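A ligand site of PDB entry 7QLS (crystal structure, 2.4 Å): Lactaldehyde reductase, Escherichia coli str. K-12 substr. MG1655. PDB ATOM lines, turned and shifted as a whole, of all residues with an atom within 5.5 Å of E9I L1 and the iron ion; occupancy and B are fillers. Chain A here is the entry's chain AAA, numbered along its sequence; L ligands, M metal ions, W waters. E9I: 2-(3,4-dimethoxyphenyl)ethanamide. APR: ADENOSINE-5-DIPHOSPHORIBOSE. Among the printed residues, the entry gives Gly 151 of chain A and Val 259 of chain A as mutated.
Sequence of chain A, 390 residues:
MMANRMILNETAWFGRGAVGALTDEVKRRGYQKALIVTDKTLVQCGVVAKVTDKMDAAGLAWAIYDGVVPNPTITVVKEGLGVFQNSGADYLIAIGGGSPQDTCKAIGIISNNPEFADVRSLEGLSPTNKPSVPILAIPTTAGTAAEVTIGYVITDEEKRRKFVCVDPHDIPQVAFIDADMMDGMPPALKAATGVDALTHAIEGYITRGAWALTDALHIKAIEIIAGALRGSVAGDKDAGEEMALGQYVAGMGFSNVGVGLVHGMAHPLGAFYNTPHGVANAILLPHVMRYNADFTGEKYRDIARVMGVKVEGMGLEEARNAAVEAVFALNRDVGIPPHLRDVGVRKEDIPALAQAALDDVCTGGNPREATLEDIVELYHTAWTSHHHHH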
ATOM      1  N   THR A 144      -2.721 -28.449  22.171  1.00  0.00           N
ATOM      2  CA  THR A 144      -1.918 -27.638  23.118  1.00  0.00           C
ATOM      3  C   THR A 144      -1.287 -28.506  24.198  1.00  0.00           C
ATOM      4  O   THR A 144      -0.301 -28.070  24.783  1.00  0.00           O
ATOM      5  CB  THR A 144      -2.724 -26.503  23.773  1.00  0.00           C
ATOM      6  OG1 THR A 144      -3.689 -27.090  24.649  1.00  0.00           O
ATOM      7  CG2 THR A 144      -3.409 -25.621  22.752  1.00  0.00           C
ATOM      8  N   THR A 149       0.477 -30.235  30.809  1.00  0.00           N
ATOM      9  CA  THR A 149       1.537 -29.207  31.065  1.00  0.00           C
ATOM     10  C   THR A 149       1.213 -28.423  32.342  1.00  0.00           C
ATOM     11  O   THR A 149       0.017 -28.370  32.702  1.00  0.00           O
ATOM     12  CB  THR A 149       1.705 -28.275  29.862  1.00  0.00           C
ATOM     13  OG1 THR A 149       0.543 -27.440  29.785  1.00  0.00           O
ATOM     14  CG2 THR A 149       1.919 -29.004  28.557  1.00  0.00           C
ATOM     15  N   ILE A 150       2.230 -27.838  32.996  1.00  0.00           N
ATOM     16  CA  ILE A 150       2.089 -26.994  34.221  1.00  0.00           C
ATOM     17  C   ILE A 150       2.023 -25.507  33.837  1.00  0.00           C
ATOM     18  O   ILE A 150       2.217 -24.659  34.729  1.00  0.00           O
ATOM     19  CB  ILE A 150       3.213 -27.255  35.257  1.00  0.00           C
ATOM     20  CG1 ILE A 150       4.607 -26.988  34.675  1.00  0.00           C
ATOM     21  CG2 ILE A 150       3.092 -28.664  35.819  1.00  0.00           C
ATOM     22  CD1 ILE A 150       5.683 -26.815  35.725  1.00  0.00           C
ATOM     23  N   GLY A 151       1.722 -25.212  32.566  1.00  0.00           N
ATOM     24  CA  GLY A 151       1.655 -23.846  32.014  1.00  0.00           C
ATOM     25  C   GLY A 151       0.247 -23.477  31.562  1.00  0.00           C
ATOM     26  O   GLY A 151      -0.534 -24.394  31.179  1.00  0.00           O
ATOM     27  N   TYR A 152      -0.085 -22.182  31.600  1.00  0.00           N
ATOM     28  CA  TYR A 152      -1.284 -21.597  30.967  1.00  0.00           C
ATOM     29  C   TYR A 152      -0.979 -20.163  30.528  1.00  0.00           C
ATOM     30  O   TYR A 152      -0.172 -19.470  31.194  1.00  0.00           O
ATOM     31  CB  TYR A 152      -2.512 -21.699  31.888  1.00  0.00           C
ATOM     32  CG  TYR A 152      -2.379 -21.141  33.284  1.00  0.00           C
ATOM     33  CD1 TYR A 152      -1.659 -21.808  34.261  1.00  0.00           C
ATOM     34  CD2 TYR A 152      -3.046 -19.987  33.656  1.00  0.00           C
ATOM     35  CE1 TYR A 152      -1.571 -21.321  35.557  1.00  0.00           C
ATOM     36  CE2 TYR A 152      -2.970 -19.480  34.946  1.00  0.00           C
ATOM     37  CZ  TYR A 152      -2.229 -20.146  35.900  1.00  0.00           C
ATOM     38  OH  TYR A 152      -2.141 -19.659  37.165  1.00  0.00           O
ATOM     39  N   VAL A 153      -1.584 -19.742  29.419  1.00  0.00           N
ATOM     40  CA  VAL A 153      -1.277 -18.450  28.751  1.00  0.00           C
ATOM     41  C   VAL A 153      -2.557 -17.597  28.727  1.00  0.00           C
ATOM     42  O   VAL A 153      -3.564 -18.019  28.116  1.00  0.00           O
ATOM     43  CB  VAL A 153      -0.674 -18.677  27.347  1.00  0.00           C
ATOM     44  CG1 VAL A 153      -0.231 -17.386  26.711  1.00  0.00           C
ATOM     45  CG2 VAL A 153       0.482 -19.651  27.418  1.00  0.00           C
ATOM     46  N   VAL A 164       2.761 -16.029  30.293  1.00  0.00           N
ATOM     47  CA  VAL A 164       2.824 -17.471  30.655  1.00  0.00           C
ATOM     48  C   VAL A 164       2.919 -17.597  32.178  1.00  0.00           C
ATOM     49  O   VAL A 164       3.786 -16.931  32.782  1.00  0.00           O
ATOM     50  CB  VAL A 164       3.993 -18.152  29.940  1.00  0.00           C
ATOM     51  CG1 VAL A 164       4.042 -19.646  30.237  1.00  0.00           C
ATOM     52  CG2 VAL A 164       3.946 -17.896  28.437  1.00  0.00           C
ATOM     53  N   VAL A 166       3.446 -20.537  35.177  1.00  0.00           N
ATOM     54  CA  VAL A 166       4.054 -21.893  35.316  1.00  0.00           C
ATOM     55  C   VAL A 166       3.979 -22.295  36.792  1.00  0.00           C
ATOM     56  O   VAL A 166       4.516 -21.566  37.646  1.00  0.00           O
ATOM     57  CB  VAL A 166       5.513 -21.911  34.789  1.00  0.00           C
ATOM     58  CG1 VAL A 166       6.155 -23.278  34.967  1.00  0.00           C
ATOM     59  CG2 VAL A 166       5.577 -21.480  33.334  1.00  0.00           C
ATOM     60  N   ASP A 196       0.986 -26.846  16.088  1.00  0.00           N
ATOM     61  CA  ASP A 196       1.311 -26.349  17.450  1.00  0.00           C
ATOM     62  C   ASP A 196       1.943 -27.509  18.232  1.00  0.00           C
ATOM     63  O   ASP A 196       3.000 -27.295  18.866  1.00  0.00           O
ATOM     64  CB  ASP A 196       0.087 -25.712  18.115  1.00  0.00           C
ATOM     65  CG  ASP A 196       0.295 -25.260  19.558  1.00  0.00           C
ATOM     66  OD1 ASP A 196       1.371 -24.715  19.863  1.00  0.00           O
ATOM     67  OD2 ASP A 196      -0.646 -25.442  20.356  1.00  0.00           O
ATOM     68  N   HIS A 200       5.847 -27.762  19.640  1.00  0.00           N
ATOM     69  CA  HIS A 200       6.152 -28.187  21.029  1.00  0.00           C
ATOM     70  C   HIS A 200       7.208 -29.287  21.014  1.00  0.00           C
ATOM     71  O   HIS A 200       8.147 -29.227  21.818  1.00  0.00           O
ATOM     72  CB  HIS A 200       4.892 -28.710  21.735  1.00  0.00           C
ATOM     73  CG  HIS A 200       3.894 -27.652  22.015  1.00  0.00           C
ATOM     74  ND1 HIS A 200       2.552 -27.919  22.019  1.00  0.00           N
ATOM     75  CD2 HIS A 200       4.037 -26.341  22.292  1.00  0.00           C
ATOM     76  CE1 HIS A 200       1.894 -26.807  22.301  1.00  0.00           C
ATOM     77  NE2 HIS A 200       2.784 -25.825  22.469  1.00  0.00           N
ATOM     78  N   PHE A 254       7.817 -30.983  26.906  1.00  0.00           N
ATOM     79  CA  PHE A 254       8.185 -29.545  26.807  1.00  0.00           C
ATOM     80  C   PHE A 254       7.798 -28.836  28.098  1.00  0.00           C
ATOM     81  O   PHE A 254       8.567 -27.973  28.537  1.00  0.00           O
ATOM     82  CB  PHE A 254       7.577 -28.907  25.557  1.00  0.00           C
ATOM     83  CG  PHE A 254       6.147 -28.444  25.657  1.00  0.00           C
ATOM     84  CD1 PHE A 254       5.832 -27.219  26.210  1.00  0.00           C
ATOM     85  CD2 PHE A 254       5.123 -29.202  25.114  1.00  0.00           C
ATOM     86  CE1 PHE A 254       4.527 -26.772  26.264  1.00  0.00           C
ATOM     87  CE2 PHE A 254       3.810 -28.757  25.161  1.00  0.00           C
ATOM     88  CZ  PHE A 254       3.509 -27.543  25.748  1.00  0.00           C
ATOM     89  N   SER A 255       6.670 -29.222  28.713  1.00  0.00           N
ATOM     90  CA  SER A 255       6.207 -28.709  30.030  1.00  0.00           C
ATOM     91  C   SER A 255       7.372 -28.698  31.032  1.00  0.00           C
ATOM     92  O   SER A 255       7.490 -27.737  31.801  1.00  0.00           O
ATOM     93  CB  SER A 255       5.053 -29.548  30.552  1.00  0.00           C
ATOM     94  OG  SER A 255       4.714 -29.219  31.893  1.00  0.00           O
ATOM     95  N   GLY A 258      11.044 -26.946  28.553  1.00  0.00           N
ATOM     96  CA  GLY A 258      10.817 -25.664  27.866  1.00  0.00           C
ATOM     97  C   GLY A 258      10.658 -25.814  26.356  1.00  0.00           C
ATOM     98  O   GLY A 258      10.764 -26.931  25.844  1.00  0.00           O
ATOM     99  N   VAL A 259      10.415 -24.696  25.680  1.00  0.00           N
ATOM    100  CA  VAL A 259      10.325 -24.588  24.199  1.00  0.00           C
ATOM    101  C   VAL A 259      11.373 -23.540  23.762  1.00  0.00           C
ATOM    102  O   VAL A 259      12.542 -23.669  24.199  1.00  0.00           O
ATOM    103  CB  VAL A 259       8.884 -24.273  23.767  1.00  0.00           C
ATOM    104  CG1 VAL A 259       8.008 -25.512  23.811  1.00  0.00           C
ATOM    105  CG2 VAL A 259       8.264 -23.162  24.584  1.00  0.00           C
ATOM    106  N   HIS A 263       7.445 -20.046  19.937  1.00  0.00           N
ATOM    107  CA  HIS A 263       6.392 -19.684  20.931  1.00  0.00           C
ATOM    108  C   HIS A 263       6.595 -18.239  21.399  1.00  0.00           C
ATOM    109  O   HIS A 263       5.580 -17.541  21.584  1.00  0.00           O
ATOM    110  CB  HIS A 263       6.377 -20.704  22.074  1.00  0.00           C
ATOM    111  CG  HIS A 263       5.462 -21.846  21.804  1.00  0.00           C
ATOM    112  ND1 HIS A 263       5.739 -22.801  20.848  1.00  0.00           N
ATOM    113  CD2 HIS A 263       4.254 -22.156  22.308  1.00  0.00           C
ATOM    114  CE1 HIS A 263       4.743 -23.659  20.800  1.00  0.00           C
ATOM    115  NE2 HIS A 263       3.823 -23.292  21.690  1.00  0.00           N
ATOM    116  N   HIS A 267       3.419 -15.557  20.532  1.00  0.00           N
ATOM    117  CA  HIS A 267       2.582 -14.963  21.610  1.00  0.00           C
ATOM    118  C   HIS A 267       2.244 -13.511  21.297  1.00  0.00           C
ATOM    119  O   HIS A 267       1.091 -13.123  21.437  1.00  0.00           O
ATOM    120  CB  HIS A 267       3.237 -15.157  22.992  1.00  0.00           C
ATOM    121  CG  HIS A 267       3.143 -16.559  23.490  1.00  0.00           C
ATOM    122  ND1 HIS A 267       3.779 -16.964  24.653  1.00  0.00           N
ATOM    123  CD2 HIS A 267       2.492 -17.642  22.999  1.00  0.00           C
ATOM    124  CE1 HIS A 267       3.521 -18.241  24.849  1.00  0.00           C
ATOM    125  NE2 HIS A 267       2.739 -18.684  23.837  1.00  0.00           N
ATOM    126  N   HIS A 277      -2.922 -19.359  17.702  1.00  0.00           N
ATOM    127  CA  HIS A 277      -1.596 -19.784  18.215  1.00  0.00           C
ATOM    128  C   HIS A 277      -0.910 -20.771  17.248  1.00  0.00           C
ATOM    129  O   HIS A 277       0.295 -20.603  16.978  1.00  0.00           O
ATOM    130  CB  HIS A 277      -1.790 -20.368  19.624  1.00  0.00           C
ATOM    131  CG  HIS A 277      -0.556 -20.944  20.230  1.00  0.00           C
ATOM    132  ND1 HIS A 277       0.518 -20.158  20.618  1.00  0.00           N
ATOM    133  CD2 HIS A 277      -0.235 -22.207  20.562  1.00  0.00           C
ATOM    134  CE1 HIS A 277       1.441 -20.913  21.144  1.00  0.00           C
ATOM    135  NE2 HIS A 277       1.002 -22.181  21.130  1.00  0.00           N
ATOM    136  N   ASN A 281       2.603 -20.174  15.069  1.00  0.00           N
ATOM    137  CA  ASN A 281       3.680 -21.183  15.298  1.00  0.00           C
ATOM    138  C   ASN A 281       4.089 -21.803  13.961  1.00  0.00           C
ATOM    139  O   ASN A 281       5.295 -21.926  13.744  1.00  0.00           O
ATOM    140  CB  ASN A 281       3.262 -22.290  16.259  1.00  0.00           C
ATOM    141  CG  ASN A 281       3.415 -21.893  17.716  1.00  0.00           C
ATOM    142  OD1 ASN A 281       4.165 -20.991  18.046  1.00  0.00           O
ATOM    143  ND2 ASN A 281       2.705 -22.565  18.600  1.00  0.00           N
ATOM    144  N   VAL A 361       8.718 -15.391  28.216  1.00  0.00           N
ATOM    145  CA  VAL A 361       9.323 -16.471  29.040  1.00  0.00           C
ATOM    146  C   VAL A 361       9.938 -17.539  28.126  1.00  0.00           C
ATOM    147  O   VAL A 361      11.032 -18.041  28.446  1.00  0.00           O
ATOM    148  CB  VAL A 361       8.285 -17.100  29.993  1.00  0.00           C
ATOM    149  CG1 VAL A 361       8.764 -18.406  30.616  1.00  0.00           C
ATOM    150  CG2 VAL A 361       7.827 -16.132  31.089  1.00  0.00           C
ATOM    151  N   CYS A 362       9.248 -17.900  27.037  1.00  0.00           N
ATOM    152  CA  CYS A 362       9.592 -19.053  26.143  1.00  0.00           C
ATOM    153  C   CYS A 362      10.976 -18.875  25.517  1.00  0.00           C
ATOM    154  O   CYS A 362      11.643 -19.907  25.253  1.00  0.00           O
ATOM    155  CB  CYS A 362       8.544 -19.228  25.063  1.00  0.00           C
ATOM    156  SG  CYS A 362       6.924 -19.712  25.723  1.00  0.00           S
HETATM  157  N1  E9I L   1       1.606 -24.925  25.597  1.00  0.00           N
HETATM  158  C7  E9I L   1       5.933 -22.561  27.300  1.00  0.00           C
HETATM  159  C8  E9I L   1       1.999 -23.698  25.291  1.00  0.00           C
HETATM  160  C9  E9I L   1       4.498 -25.673  30.445  1.00  0.00           C
HETATM  161  O1  E9I L   1       4.984 -24.336  30.299  1.00  0.00           O
HETATM  162  C1  E9I L   1       3.551 -22.974  27.184  1.00  0.00           C
HETATM  163  C5  E9I L   1       4.715 -22.453  26.633  1.00  0.00           C
HETATM  164  C6  E9I L   1       5.986 -23.201  28.520  1.00  0.00           C
HETATM  165  C4  E9I L   1       4.819 -23.750  29.080  1.00  0.00           C
HETATM  166  C3  E9I L   1       3.616 -23.638  28.397  1.00  0.00           C
HETATM  167  O3  E9I L   1       2.178 -23.315  24.130  1.00  0.00           O
HETATM  168  C2  E9I L   1       2.215 -22.763  26.505  1.00  0.00           C
HETATM  169  O2  E9I L   1       7.130 -23.350  29.264  1.00  0.00           O
HETATM  170  C10 E9I L   1       7.877 -22.182  29.564  1.00  0.00           C
HETATM  171  N1  APR L   2     -14.878 -28.751  17.384  1.00  0.00           N
HETATM  172  C2  APR L   2     -15.184 -27.524  16.951  1.00  0.00           C
HETATM  173  N3  APR L   2     -14.649 -26.349  17.275  1.00  0.00           N
HETATM  174  C4  APR L   2     -13.680 -26.510  18.188  1.00  0.00           C
HETATM  175  C5  APR L   2     -13.255 -27.699  18.737  1.00  0.00           C
HETATM  176  C6  APR L   2     -13.885 -28.879  18.308  1.00  0.00           C
HETATM  177  N6  APR L   2     -13.578 -30.097  18.738  1.00  0.00           N
HETATM  178  N7  APR L   2     -12.225 -27.464  19.642  1.00  0.00           N
HETATM  179  C8  APR L   2     -12.053 -26.160  19.627  1.00  0.00           C
HETATM  180  N9  APR L   2     -12.917 -25.527  18.759  1.00  0.00           N
HETATM  181  C1' APR L   2     -13.001 -24.091  18.468  1.00  0.00           C
HETATM  182  C2' APR L   2     -13.166 -23.212  19.697  1.00  0.00           C
HETATM  183  O2' APR L   2     -14.530 -23.132  20.057  1.00  0.00           O
HETATM  184  C3' APR L   2     -12.610 -21.879  19.183  1.00  0.00           C
HETATM  185  O3' APR L   2     -13.612 -21.167  18.481  1.00  0.00           O
HETATM  186  O4' APR L   2     -11.785 -23.686  17.871  1.00  0.00           O
HETATM  187  C4' APR L   2     -11.472 -22.325  18.249  1.00  0.00           C
HETATM  188  C5' APR L   2     -10.082 -22.264  18.834  1.00  0.00           C
HETATM  189  O5' APR L   2     -10.068 -22.887  20.155  1.00  0.00           O
HETATM  190  PA  APR L   2      -8.805 -22.738  21.121  1.00  0.00           P
HETATM  191  O1A APR L   2      -9.112 -23.373  22.442  1.00  0.00           O
HETATM  192  O2A APR L   2      -8.317 -21.325  21.106  1.00  0.00           O
HETATM  193  O3A APR L   2      -7.711 -23.665  20.381  1.00  0.00           O
HETATM  194  PB  APR L   2      -6.259 -24.166  20.831  1.00  0.00           P
HETATM  195  O1B APR L   2      -6.396 -25.519  21.427  1.00  0.00           O
HETATM  196  O2B APR L   2      -5.310 -23.976  19.686  1.00  0.00           O
HETATM  197  O5D APR L   2      -5.892 -23.137  21.989  1.00  0.00           O
HETATM  198  C5D APR L   2      -4.736 -22.277  21.871  1.00  0.00           C
HETATM  199  O4D APR L   2      -3.778 -22.303  24.077  1.00  0.00           O
HETATM  200  O1D APR L   2      -1.502 -22.501  24.426  1.00  0.00           O
HETATM  201  C1D APR L   2      -2.573 -21.620  24.418  1.00  0.00           C
HETATM  202  O2D APR L   2      -1.629 -19.417  23.733  1.00  0.00           O
HETATM  203  C2D APR L   2      -2.408 -20.536  23.350  1.00  0.00           C
HETATM  204  O3D APR L   2      -4.434 -19.226  23.967  1.00  0.00           O
HETATM  205  C3D APR L   2      -3.869 -20.154  23.046  1.00  0.00           C
HETATM  206  C4D APR L   2      -4.564 -21.514  23.159  1.00  0.00           C
HETATM  207 FE    FE M   1       1.822 -23.945  21.903  1.00  0.00          FE
HETATM  208  O   HOH W   1      -0.124 -24.504  22.628  1.00  0.00           O
HETATM  209  O   HOH W   2       0.738 -20.715  24.147  1.00  0.00           O
HETATM  210  O   HOH W   3      -0.104 -26.183  27.074  1.00  0.00           O
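A ring nitrogen (NE2) of His 277 lies close to the side-chain amide nitrogen (ND2) of Asn 281, at 3.1 Å.
NE2 of His 263 lies close to ND2 of Asn 281 (3.4 Å).
The side-chain carboxylate of Asp 196 lies close to the side-chain amide nitrogen of Asn 281, 2.8 Å away.
N of Ile 150 lies within hydrogen-bond range of OG of Ser 255.
Thr 144 touches E9I L1 (O to N1, 3.8 Å).
Thr 149 touches E9I L1 (CB to C9, 3.9 Å).
Gly 151 touches E9I L1 (N to C9, 3.5 Å).
Val 153 touches E9I L1.
Phe 254 touches E9I L1.
Ser 255 touches E9I L1.
Val 259 touches E9I L1 (CG2 to C7, 3.6 Å).
Cys 362 touches E9I L1.
Of the 20 residues printed, 11 come within 4 Å of E9I L1.
Asn 281 touches the iron ion (ND2 to FE, 3.7 Å).
Within 4 Å of the iron ion: Asp 196, His 200, His 263, His 277 and Asn 281.
The iron ion is bound by a ring nitrogen (NE2) of His 277 (2.1 Å), a ring nitrogen (NE2) of His 263 (2.1 Å), water W1 (2.2 Å), a ring nitrogen (NE2) of His 200 (2.2 Å), the side-chain carboxylate of Asp 196 (2.2 Å) and an oxygen (O3) of E9I L1 (2.3 Å).
The iron ion has six donor atoms within binding distance.
Water W1 lies within hydrogen-bond range of the side-chain carboxylate (OD2) of Asp 196, an oxygen (O1D) of APR L2 and a nitrogen (N1) of E9I L1.
Water W3 lies within hydrogen-bond range of N1 of E9I L1 (2.6 Å), O of Thr 144 (3.0 Å) and OG1 of Thr 149 (3.1 Å).
Water W2 bridges O2D of APR L2 and NE2 of His 267.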
